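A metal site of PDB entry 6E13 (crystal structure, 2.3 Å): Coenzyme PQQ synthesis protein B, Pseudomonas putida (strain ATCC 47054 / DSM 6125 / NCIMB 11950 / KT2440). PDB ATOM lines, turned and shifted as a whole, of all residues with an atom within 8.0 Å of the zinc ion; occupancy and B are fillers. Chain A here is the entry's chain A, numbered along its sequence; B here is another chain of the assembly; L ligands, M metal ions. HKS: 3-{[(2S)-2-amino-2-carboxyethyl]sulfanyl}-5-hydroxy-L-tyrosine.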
ATOM      1  N   GLY A  14      24.804  21.309  12.121  1.00  0.00           N
ATOM      2  CA  GLY A  14      25.807  21.827  11.208  1.00  0.00           C
ATOM      3  C   GLY A  14      25.706  23.340  11.068  1.00  0.00           C
ATOM      4  O   GLY A  14      25.105  24.044  11.877  1.00  0.00           O
ATOM      5  N   PHE A  15      26.329  23.839  10.002  1.00  0.00           N
ATOM      6  CA  PHE A  15      26.170  25.261   9.698  1.00  0.00           C
ATOM      7  C   PHE A  15      26.232  25.508   8.200  1.00  0.00           C
ATOM      8  O   PHE A  15      27.242  25.185   7.558  1.00  0.00           O
ATOM      9  CB  PHE A  15      27.219  26.114  10.419  1.00  0.00           C
ATOM     10  CG  PHE A  15      27.149  27.570  10.019  1.00  0.00           C
ATOM     11  CD1 PHE A  15      26.029  28.322  10.309  1.00  0.00           C
ATOM     12  CD2 PHE A  15      28.191  28.163   9.309  1.00  0.00           C
ATOM     13  CE1 PHE A  15      25.948  29.642   9.917  1.00  0.00           C
ATOM     14  CE2 PHE A  15      28.111  29.474   8.919  1.00  0.00           C
ATOM     15  CZ  PHE A  15      26.999  30.220   9.218  1.00  0.00           C
ATOM     16  N   PRO A  16      25.171  26.070   7.607  1.00  0.00           N
ATOM     17  CA  PRO A  16      23.913  26.408   8.273  1.00  0.00           C
ATOM     18  C   PRO A  16      23.093  25.185   8.675  1.00  0.00           C
ATOM     19  O   PRO A  16      23.261  24.095   8.091  1.00  0.00           O
ATOM     20  CB  PRO A  16      23.154  27.203   7.212  1.00  0.00           C
ATOM     21  CG  PRO A  16      23.638  26.589   5.909  1.00  0.00           C
ATOM     22  CD  PRO A  16      25.102  26.282   6.145  1.00  0.00           C
ATOM     23  N   GLN A  17      22.215  25.361   9.651  1.00  0.00           N
ATOM     24  CA  GLN A  17      21.307  24.307  10.082  1.00  0.00           C
ATOM     25  C   GLN A  17      20.040  24.333   9.226  1.00  0.00           C
ATOM     26  O   GLN A  17      19.490  25.400   8.939  1.00  0.00           O
ATOM     27  CB  GLN A  17      20.964  24.466  11.563  1.00  0.00           C
ATOM     28  CG  GLN A  17      20.035  23.421  12.136  1.00  0.00           C
ATOM     29  CD  GLN A  17      20.048  23.467  13.674  1.00  0.00           C
ATOM     30  OE1 GLN A  17      21.122  23.392  14.288  1.00  0.00           O
ATOM     31  NE2 GLN A  17      18.872  23.600  14.290  1.00  0.00           N
ATOM     32  N   TRP A  18      19.575  23.132   8.856  1.00  0.00           N
ATOM     33  CA  TRP A  18      18.551  22.993   7.829  1.00  0.00           C
ATOM     34  C   TRP A  18      17.308  23.833   8.099  1.00  0.00           C
ATOM     35  O   TRP A  18      16.694  24.360   7.167  1.00  0.00           O
ATOM     36  CB  TRP A  18      18.174  21.505   7.676  1.00  0.00           C
ATOM     37  CG  TRP A  18      17.530  20.942   8.886  1.00  0.00           C
ATOM     38  CD1 TRP A  18      18.147  20.528  10.025  1.00  0.00           C
ATOM     39  CD2 TRP A  18      16.124  20.731   9.099  1.00  0.00           C
ATOM     40  NE1 TRP A  18      17.223  20.086  10.934  1.00  0.00           N
ATOM     41  CE2 TRP A  18      15.973  20.210  10.391  1.00  0.00           C
ATOM     42  CE3 TRP A  18      14.979  20.950   8.310  1.00  0.00           C
ATOM     43  CZ2 TRP A  18      14.730  19.884  10.925  1.00  0.00           C
ATOM     44  CZ3 TRP A  18      13.748  20.635   8.841  1.00  0.00           C
ATOM     45  CH2 TRP A  18      13.635  20.100  10.132  1.00  0.00           C
ATOM     46  N   ASN A  19      16.908  23.983   9.367  1.00  0.00           N
ATOM     47  CA  ASN A  19      15.635  24.623   9.687  1.00  0.00           C
ATOM     48  C   ASN A  19      15.811  25.977  10.387  1.00  0.00           C
ATOM     49  O   ASN A  19      14.846  26.501  10.965  1.00  0.00           O
ATOM     50  CB  ASN A  19      14.768  23.709  10.547  1.00  0.00           C
ATOM     51  CG  ASN A  19      15.296  23.551  11.949  1.00  0.00           C
ATOM     52  OD1 ASN A  19      16.497  23.668  12.186  1.00  0.00           O
ATOM     53  ND2 ASN A  19      14.415  23.261  12.899  1.00  0.00           N
ATOM     54  N   CYS A  20      17.002  26.563  10.321  1.00  0.00           N
ATOM     55  CA  CYS A  20      17.338  27.731  11.133  1.00  0.00           C
ATOM     56  C   CYS A  20      17.525  28.950  10.252  1.00  0.00           C
ATOM     57  O   CYS A  20      18.237  28.906   9.250  1.00  0.00           O
ATOM     58  CB  CYS A  20      18.622  27.496  11.929  1.00  0.00           C
ATOM     59  SG  CYS A  20      19.003  28.895  13.018  1.00  0.00           S
ATOM     60  N   ASN A  21      16.906  30.057  10.663  1.00  0.00           N
ATOM     61  CA  ASN A  21      17.075  31.345   9.997  1.00  0.00           C
ATOM     62  C   ASN A  21      17.563  32.404  10.982  1.00  0.00           C
ATOM     63  O   ASN A  21      17.176  33.573  10.916  1.00  0.00           O
ATOM     64  CB  ASN A  21      15.777  31.761   9.313  1.00  0.00           C
ATOM     65  CG  ASN A  21      15.339  30.763   8.244  1.00  0.00           C
ATOM     66  OD1 ASN A  21      15.928  30.691   7.167  1.00  0.00           O
ATOM     67  ND2 ASN A  21      14.290  29.989   8.552  1.00  0.00           N
ATOM     68  N   CYS A  22      18.424  31.983  11.915  1.00  0.00           N
ATOM     69  CA  CYS A  22      19.091  32.891  12.837  1.00  0.00           C
ATOM     70  C   CYS A  22      20.026  33.813  12.052  1.00  0.00           C
ATOM     71  O   CYS A  22      20.223  33.663  10.843  1.00  0.00           O
ATOM     72  CB  CYS A  22      19.855  32.109  13.902  1.00  0.00           C
ATOM     73  SG  CYS A  22      21.552  31.577  13.376  1.00  0.00           S
ATOM     74  N   VAL A  23      20.607  34.797  12.741  1.00  0.00           N
ATOM     75  CA  VAL A  23      21.419  35.791  12.041  1.00  0.00           C
ATOM     76  C   VAL A  23      22.552  35.120  11.253  1.00  0.00           C
ATOM     77  O   VAL A  23      22.785  35.446  10.091  1.00  0.00           O
ATOM     78  CB  VAL A  23      21.924  36.871  13.015  1.00  0.00           C
ATOM     79  CG1 VAL A  23      20.760  37.470  13.787  1.00  0.00           C
ATOM     80  CG2 VAL A  23      22.931  36.309  13.996  1.00  0.00           C
ATOM     81  N   ASN A  24      23.217  34.119  11.860  1.00  0.00           N
ATOM     82  CA  ASN A  24      24.301  33.431  11.168  1.00  0.00           C
ATOM     83  C   ASN A  24      23.814  32.649   9.946  1.00  0.00           C
ATOM     84  O   ASN A  24      24.368  32.775   8.851  1.00  0.00           O
ATOM     85  CB  ASN A  24      25.020  32.478  12.116  1.00  0.00           C
ATOM     86  CG  ASN A  24      26.060  33.157  12.986  1.00  0.00           C
ATOM     87  OD1 ASN A  24      26.518  34.257  12.680  1.00  0.00           O
ATOM     88  ND2 ASN A  24      26.451  32.485  14.081  1.00  0.00           N
ATOM     89  N   CYS A  25      22.771  31.825  10.127  1.00  0.00           N
ATOM     90  CA  CYS A  25      22.369  30.904   9.051  1.00  0.00           C
ATOM     91  C   CYS A  25      21.736  31.652   7.878  1.00  0.00           C
ATOM     92  O   CYS A  25      22.104  31.426   6.712  1.00  0.00           O
ATOM     93  CB  CYS A  25      21.416  29.839   9.598  1.00  0.00           C
ATOM     94  SG  CYS A  25      22.214  28.618  10.721  1.00  0.00           S
ATOM     95  N   LYS A  26      20.783  32.557   8.167  1.00  0.00           N
ATOM     96  CA  LYS A  26      20.203  33.394   7.109  1.00  0.00           C
ATOM     97  C   LYS A  26      21.258  34.303   6.488  1.00  0.00           C
ATOM     98  O   LYS A  26      21.273  34.493   5.269  1.00  0.00           O
ATOM     99  CB  LYS A  26      19.041  34.222   7.663  1.00  0.00           C
ATOM    100  CG  LYS A  26      18.147  34.811   6.581  1.00  0.00           C
ATOM    101  CD  LYS A  26      17.221  35.884   7.117  1.00  0.00           C
ATOM    102  CE  LYS A  26      15.825  35.785   6.528  1.00  0.00           C
ATOM    103  NZ  LYS A  26      14.943  34.813   7.284  1.00  0.00           N
ATOM    104  N   GLY A  27      22.168  34.832   7.310  1.00  0.00           N
ATOM    105  CA  GLY A  27      23.244  35.651   6.777  1.00  0.00           C
ATOM    106  C   GLY A  27      24.133  34.893   5.796  1.00  0.00           C
ATOM    107  O   GLY A  27      24.532  35.434   4.763  1.00  0.00           O
ATOM    108  N   ARG A  29      23.126  32.161   4.029  1.00  0.00           N
ATOM    109  CA  ARG A  29      22.332  31.884   2.831  1.00  0.00           C
ATOM    110  C   ARG A  29      22.121  33.153   2.012  1.00  0.00           C
ATOM    111  O   ARG A  29      22.204  33.123   0.775  1.00  0.00           O
ATOM    112  CB  ARG A  29      20.978  31.282   3.208  1.00  0.00           C
ATOM    113  CG  ARG A  29      21.022  29.861   3.774  1.00  0.00           C
ATOM    114  CD  ARG A  29      19.636  29.248   3.818  1.00  0.00           C
ATOM    115  NE  ARG A  29      19.556  28.137   4.769  1.00  0.00           N
ATOM    116  CZ  ARG A  29      19.204  28.257   6.048  1.00  0.00           C
ATOM    117  NH1 ARG A  29      19.151  27.184   6.833  1.00  0.00           N
ATOM    118  NH2 ARG A  29      18.904  29.452   6.555  1.00  0.00           N
ATOM    119  N   ARG A 233      19.226  34.443  20.422  1.00  0.00           N
ATOM    120  CA  ARG A 233      19.013  34.374  18.977  1.00  0.00           C
ATOM    121  C   ARG A 233      17.560  34.118  18.601  1.00  0.00           C
ATOM    122  O   ARG A 233      17.227  34.196  17.420  1.00  0.00           O
ATOM    123  CB  ARG A 233      19.907  33.287  18.362  1.00  0.00           C
ATOM    124  CG  ARG A 233      21.395  33.495  18.555  1.00  0.00           C
ATOM    125  CD  ARG A 233      21.922  34.656  17.710  1.00  0.00           C
ATOM    126  NE  ARG A 233      23.341  34.485  17.411  1.00  0.00           N
ATOM    127  CZ  ARG A 233      24.165  35.476  17.082  1.00  0.00           C
ATOM    128  NH1 ARG A 233      25.446  35.226  16.813  1.00  0.00           N
ATOM    129  NH2 ARG A 233      23.721  36.720  17.024  1.00  0.00           N
ATOM    130  N   VAL A 235      15.965  31.207  18.956  1.00  0.00           N
ATOM    131  CA  VAL A 235      15.823  29.888  18.337  1.00  0.00           C
ATOM    132  C   VAL A 235      15.489  28.787  19.335  1.00  0.00           C
ATOM    133  O   VAL A 235      15.170  27.662  18.914  1.00  0.00           O
ATOM    134  CB  VAL A 235      17.070  29.514  17.527  1.00  0.00           C
ATOM    135  CG1 VAL A 235      17.163  30.391  16.288  1.00  0.00           C
ATOM    136  CG2 VAL A 235      18.314  29.653  18.394  1.00  0.00           C
ATOM    137  N   ASN A 272      28.282  25.751  17.347  1.00  0.00           N
ATOM    138  CA  ASN A 272      26.879  25.780  16.954  1.00  0.00           C
ATOM    139  C   ASN A 272      26.585  26.900  15.960  1.00  0.00           C
ATOM    140  O   ASN A 272      27.246  27.947  15.942  1.00  0.00           O
ATOM    141  CB  ASN A 272      25.979  25.920  18.190  1.00  0.00           C
ATOM    142  CG  ASN A 272      24.527  25.569  17.894  1.00  0.00           C
ATOM    143  OD1 ASN A 272      24.180  24.402  17.713  1.00  0.00           O
ATOM    144  ND2 ASN A 272      23.678  26.579  17.890  1.00  0.00           N
ATOM    145  N   ASN A 273      25.566  26.660  15.123  1.00  0.00           N
ATOM    146  CA  ASN A 273      25.167  27.608  14.096  1.00  0.00           C
ATOM    147  C   ASN A 273      24.846  28.990  14.662  1.00  0.00           C
ATOM    148  O   ASN A 273      24.893  29.968  13.920  1.00  0.00           O
ATOM    149  CB  ASN A 273      23.964  27.066  13.308  1.00  0.00           C
ATOM    150  CG  ASN A 273      22.698  27.018  14.148  1.00  0.00           C
ATOM    151  OD1 ASN A 273      22.030  28.034  14.344  1.00  0.00           O
ATOM    152  ND2 ASN A 273      22.365  25.831  14.656  1.00  0.00           N
ATOM    153  N   THR A 274      24.520  29.086  15.955  1.00  0.00           N
ATOM    154  CA  THR A 274      24.171  30.379  16.553  1.00  0.00           C
ATOM    155  C   THR A 274      25.393  31.193  16.990  1.00  0.00           C
ATOM    156  O   THR A 274      25.238  32.377  17.299  1.00  0.00           O
ATOM    157  CB  THR A 274      23.267  30.187  17.756  1.00  0.00           C
ATOM    158  OG1 THR A 274      23.877  29.246  18.658  1.00  0.00           O
ATOM    159  CG2 THR A 274      21.878  29.699  17.328  1.00  0.00           C
ATOM    160  N   ASN A 275      26.583  30.597  17.040  1.00  0.00           N
ATOM    161  CA  ASN A 275      27.725  31.221  17.696  1.00  0.00           C
ATOM    162  C   ASN A 275      28.328  32.328  16.832  1.00  0.00           C
ATOM    163  O   ASN A 275      28.679  32.072  15.679  1.00  0.00           O
ATOM    164  CB  ASN A 275      28.783  30.158  18.024  1.00  0.00           C
ATOM    165  CG  ASN A 275      29.852  30.663  18.978  1.00  0.00           C
ATOM    166  OD1 ASN A 275      30.271  31.824  18.911  1.00  0.00           O
ATOM    167  ND2 ASN A 275      30.314  29.787  19.863  1.00  0.00           N
ATOM    168  N   LEU A 278      31.490  32.280  14.306  1.00  0.00           N
ATOM    169  CA  LEU A 278      31.424  31.862  12.906  1.00  0.00           C
ATOM    170  C   LEU A 278      31.408  33.062  11.964  1.00  0.00           C
ATOM    171  O   LEU A 278      31.911  32.963  10.837  1.00  0.00           O
ATOM    172  CB  LEU A 278      30.195  30.976  12.660  1.00  0.00           C
ATOM    173  CG  LEU A 278      30.108  29.655  13.433  1.00  0.00           C
ATOM    174  CD1 LEU A 278      28.770  28.981  13.189  1.00  0.00           C
ATOM    175  CD2 LEU A 278      31.264  28.715  13.072  1.00  0.00           C
ATOM    176  N   LEU B  77      12.086  32.242  12.547  1.00  0.00           N
ATOM    177  CA  LEU B  77      13.455  31.960  12.959  1.00  0.00           C
ATOM    178  C   LEU B  77      13.776  30.464  12.834  1.00  0.00           C
ATOM    179  O   LEU B  77      14.911  30.079  12.498  1.00  0.00           O
ATOM    180  CB  LEU B  77      13.671  32.453  14.389  1.00  0.00           C
ATOM    181  CG  LEU B  77      13.848  33.980  14.498  1.00  0.00           C
ATOM    182  CD1 LEU B  77      14.021  34.430  15.955  1.00  0.00           C
ATOM    183  CD2 LEU B  77      15.024  34.447  13.644  1.00  0.00           C
ATOM    184  N   ARG B  78      12.795  29.598  13.101  1.00  0.00           N
ATOM    185  CA  ARG B  78      12.870  28.187  12.772  1.00  0.00           C
ATOM    186  C   ARG B  78      11.740  27.866  11.801  1.00  0.00           C
ATOM    187  O   ARG B  78      10.577  28.180  12.079  1.00  0.00           O
ATOM    188  CB  ARG B  78      12.810  27.321  14.033  1.00  0.00           C
ATOM    189  CG  ARG B  78      14.076  27.415  14.912  1.00  0.00           C
ATOM    190  CD  ARG B  78      15.273  26.732  14.241  1.00  0.00           C
ATOM    191  NE  ARG B  78      16.607  27.206  14.654  1.00  0.00           N
ATOM    192  CZ  ARG B  78      17.387  26.598  15.565  1.00  0.00           C
ATOM    193  NH1 ARG B  78      16.969  25.500  16.200  1.00  0.00           N
ATOM    194  NH2 ARG B  78      18.579  27.080  15.850  1.00  0.00           N
HETATM  195  C02 HKS L   1      20.118  24.391  17.583  1.00  0.00           C
HETATM  196  C04 HKS L   1      20.851  23.222  18.138  1.00  0.00           C
HETATM  197  C06 HKS L   1      21.509  23.336  19.582  1.00  0.00           C
HETATM  198  C07 HKS L   1      22.224  22.017  19.915  1.00  0.00           C
HETATM  199  C08 HKS L   1      21.511  21.034  20.591  1.00  0.00           C
HETATM  200  C09 HKS L   1      22.135  19.827  20.893  1.00  0.00           C
HETATM  201  C11 HKS L   1      20.516  17.530  20.518  1.00  0.00           C
HETATM  202  C12 HKS L   1      20.439  16.137  21.112  1.00  0.00           C
HETATM  203  C13 HKS L   1      21.805  15.601  21.684  1.00  0.00           C
HETATM  204  C17 HKS L   1      23.479  19.565  20.529  1.00  0.00           C
HETATM  205  C19 HKS L   1      24.187  20.529  19.864  1.00  0.00           C
HETATM  206  C21 HKS L   1      23.566  21.764  19.549  1.00  0.00           C
HETATM  207  N05 HKS L   1      21.852  22.948  17.230  1.00  0.00           N
HETATM  208  N16 HKS L   1      19.915  15.251  20.093  1.00  0.00           N
HETATM  209  O01 HKS L   1      18.878  24.320  17.434  1.00  0.00           O
HETATM  210  O03 HKS L   1      20.743  25.415  17.226  1.00  0.00           O
HETATM  211  O14 HKS L   1      21.768  14.774  22.654  1.00  0.00           O
HETATM  212  O15 HKS L   1      22.931  15.971  21.197  1.00  0.00           O
HETATM  213  O18 HKS L   1      24.206  18.347  20.797  1.00  0.00           O
HETATM  214  O20 HKS L   1      25.528  20.193  19.546  1.00  0.00           O
HETATM  215  S10 HKS L   1      21.152  18.599  21.744  1.00  0.00           S
HETATM  216 ZN    ZN M   1      21.261  29.243  12.760  1.00  0.00          ZN
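O of Asn 273 is in hydrogen-bond range of ND2 of Asn 24 (3.0 Å). N of Gln 17 lies close to SG of Cys 25 (3.4 Å). The backbone NH (N) of Asn 24 lies close to the side-chain sulfur (SG) of Cys 22 (3.4 Å). The side-chain sulfur of Cys 20 sits close to the guanidinium group of Arg 78 of chain B (3.4 Å). NH2 of Arg 29 sits at hydrogen-bond distance from O of Cys 20 (2.8 Å). ND2 of Asn 273 sits at hydrogen-bond distance from OE1 of Gln 17 (2.8 Å).
The side-chain amide oxygen of Gln 17 is in hydrogen-bond range of a nitrogen (N05) of the ligand (3.1 Å). The side-chain amide nitrogen (ND2) of Asn 273 lies within hydrogen-bond range of an oxygen (O03) of the ligand, at 3.1 Å. NH1 of Arg 78 of chain B is in salt-bridge range of O01 of the ligand. The side-chain amide oxygen (OD1) of Asn 272 lies within hydrogen-bond range of a nitrogen (N05) of the ligand, 2.8 Å away.
OD1 of Asn 273 binds the zinc ion (2.1 Å). The side-chain sulfur (SG) of Cys 20 is bound to the zinc ion, at 2.3 Å. SG of Cys 25 is bound to the zinc ion, at 2.3 Å. The side-chain sulfur (SG) of Cys 22 is bound to the zinc ion (2.4 Å). The zinc ion has four donor atoms within binding distance.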
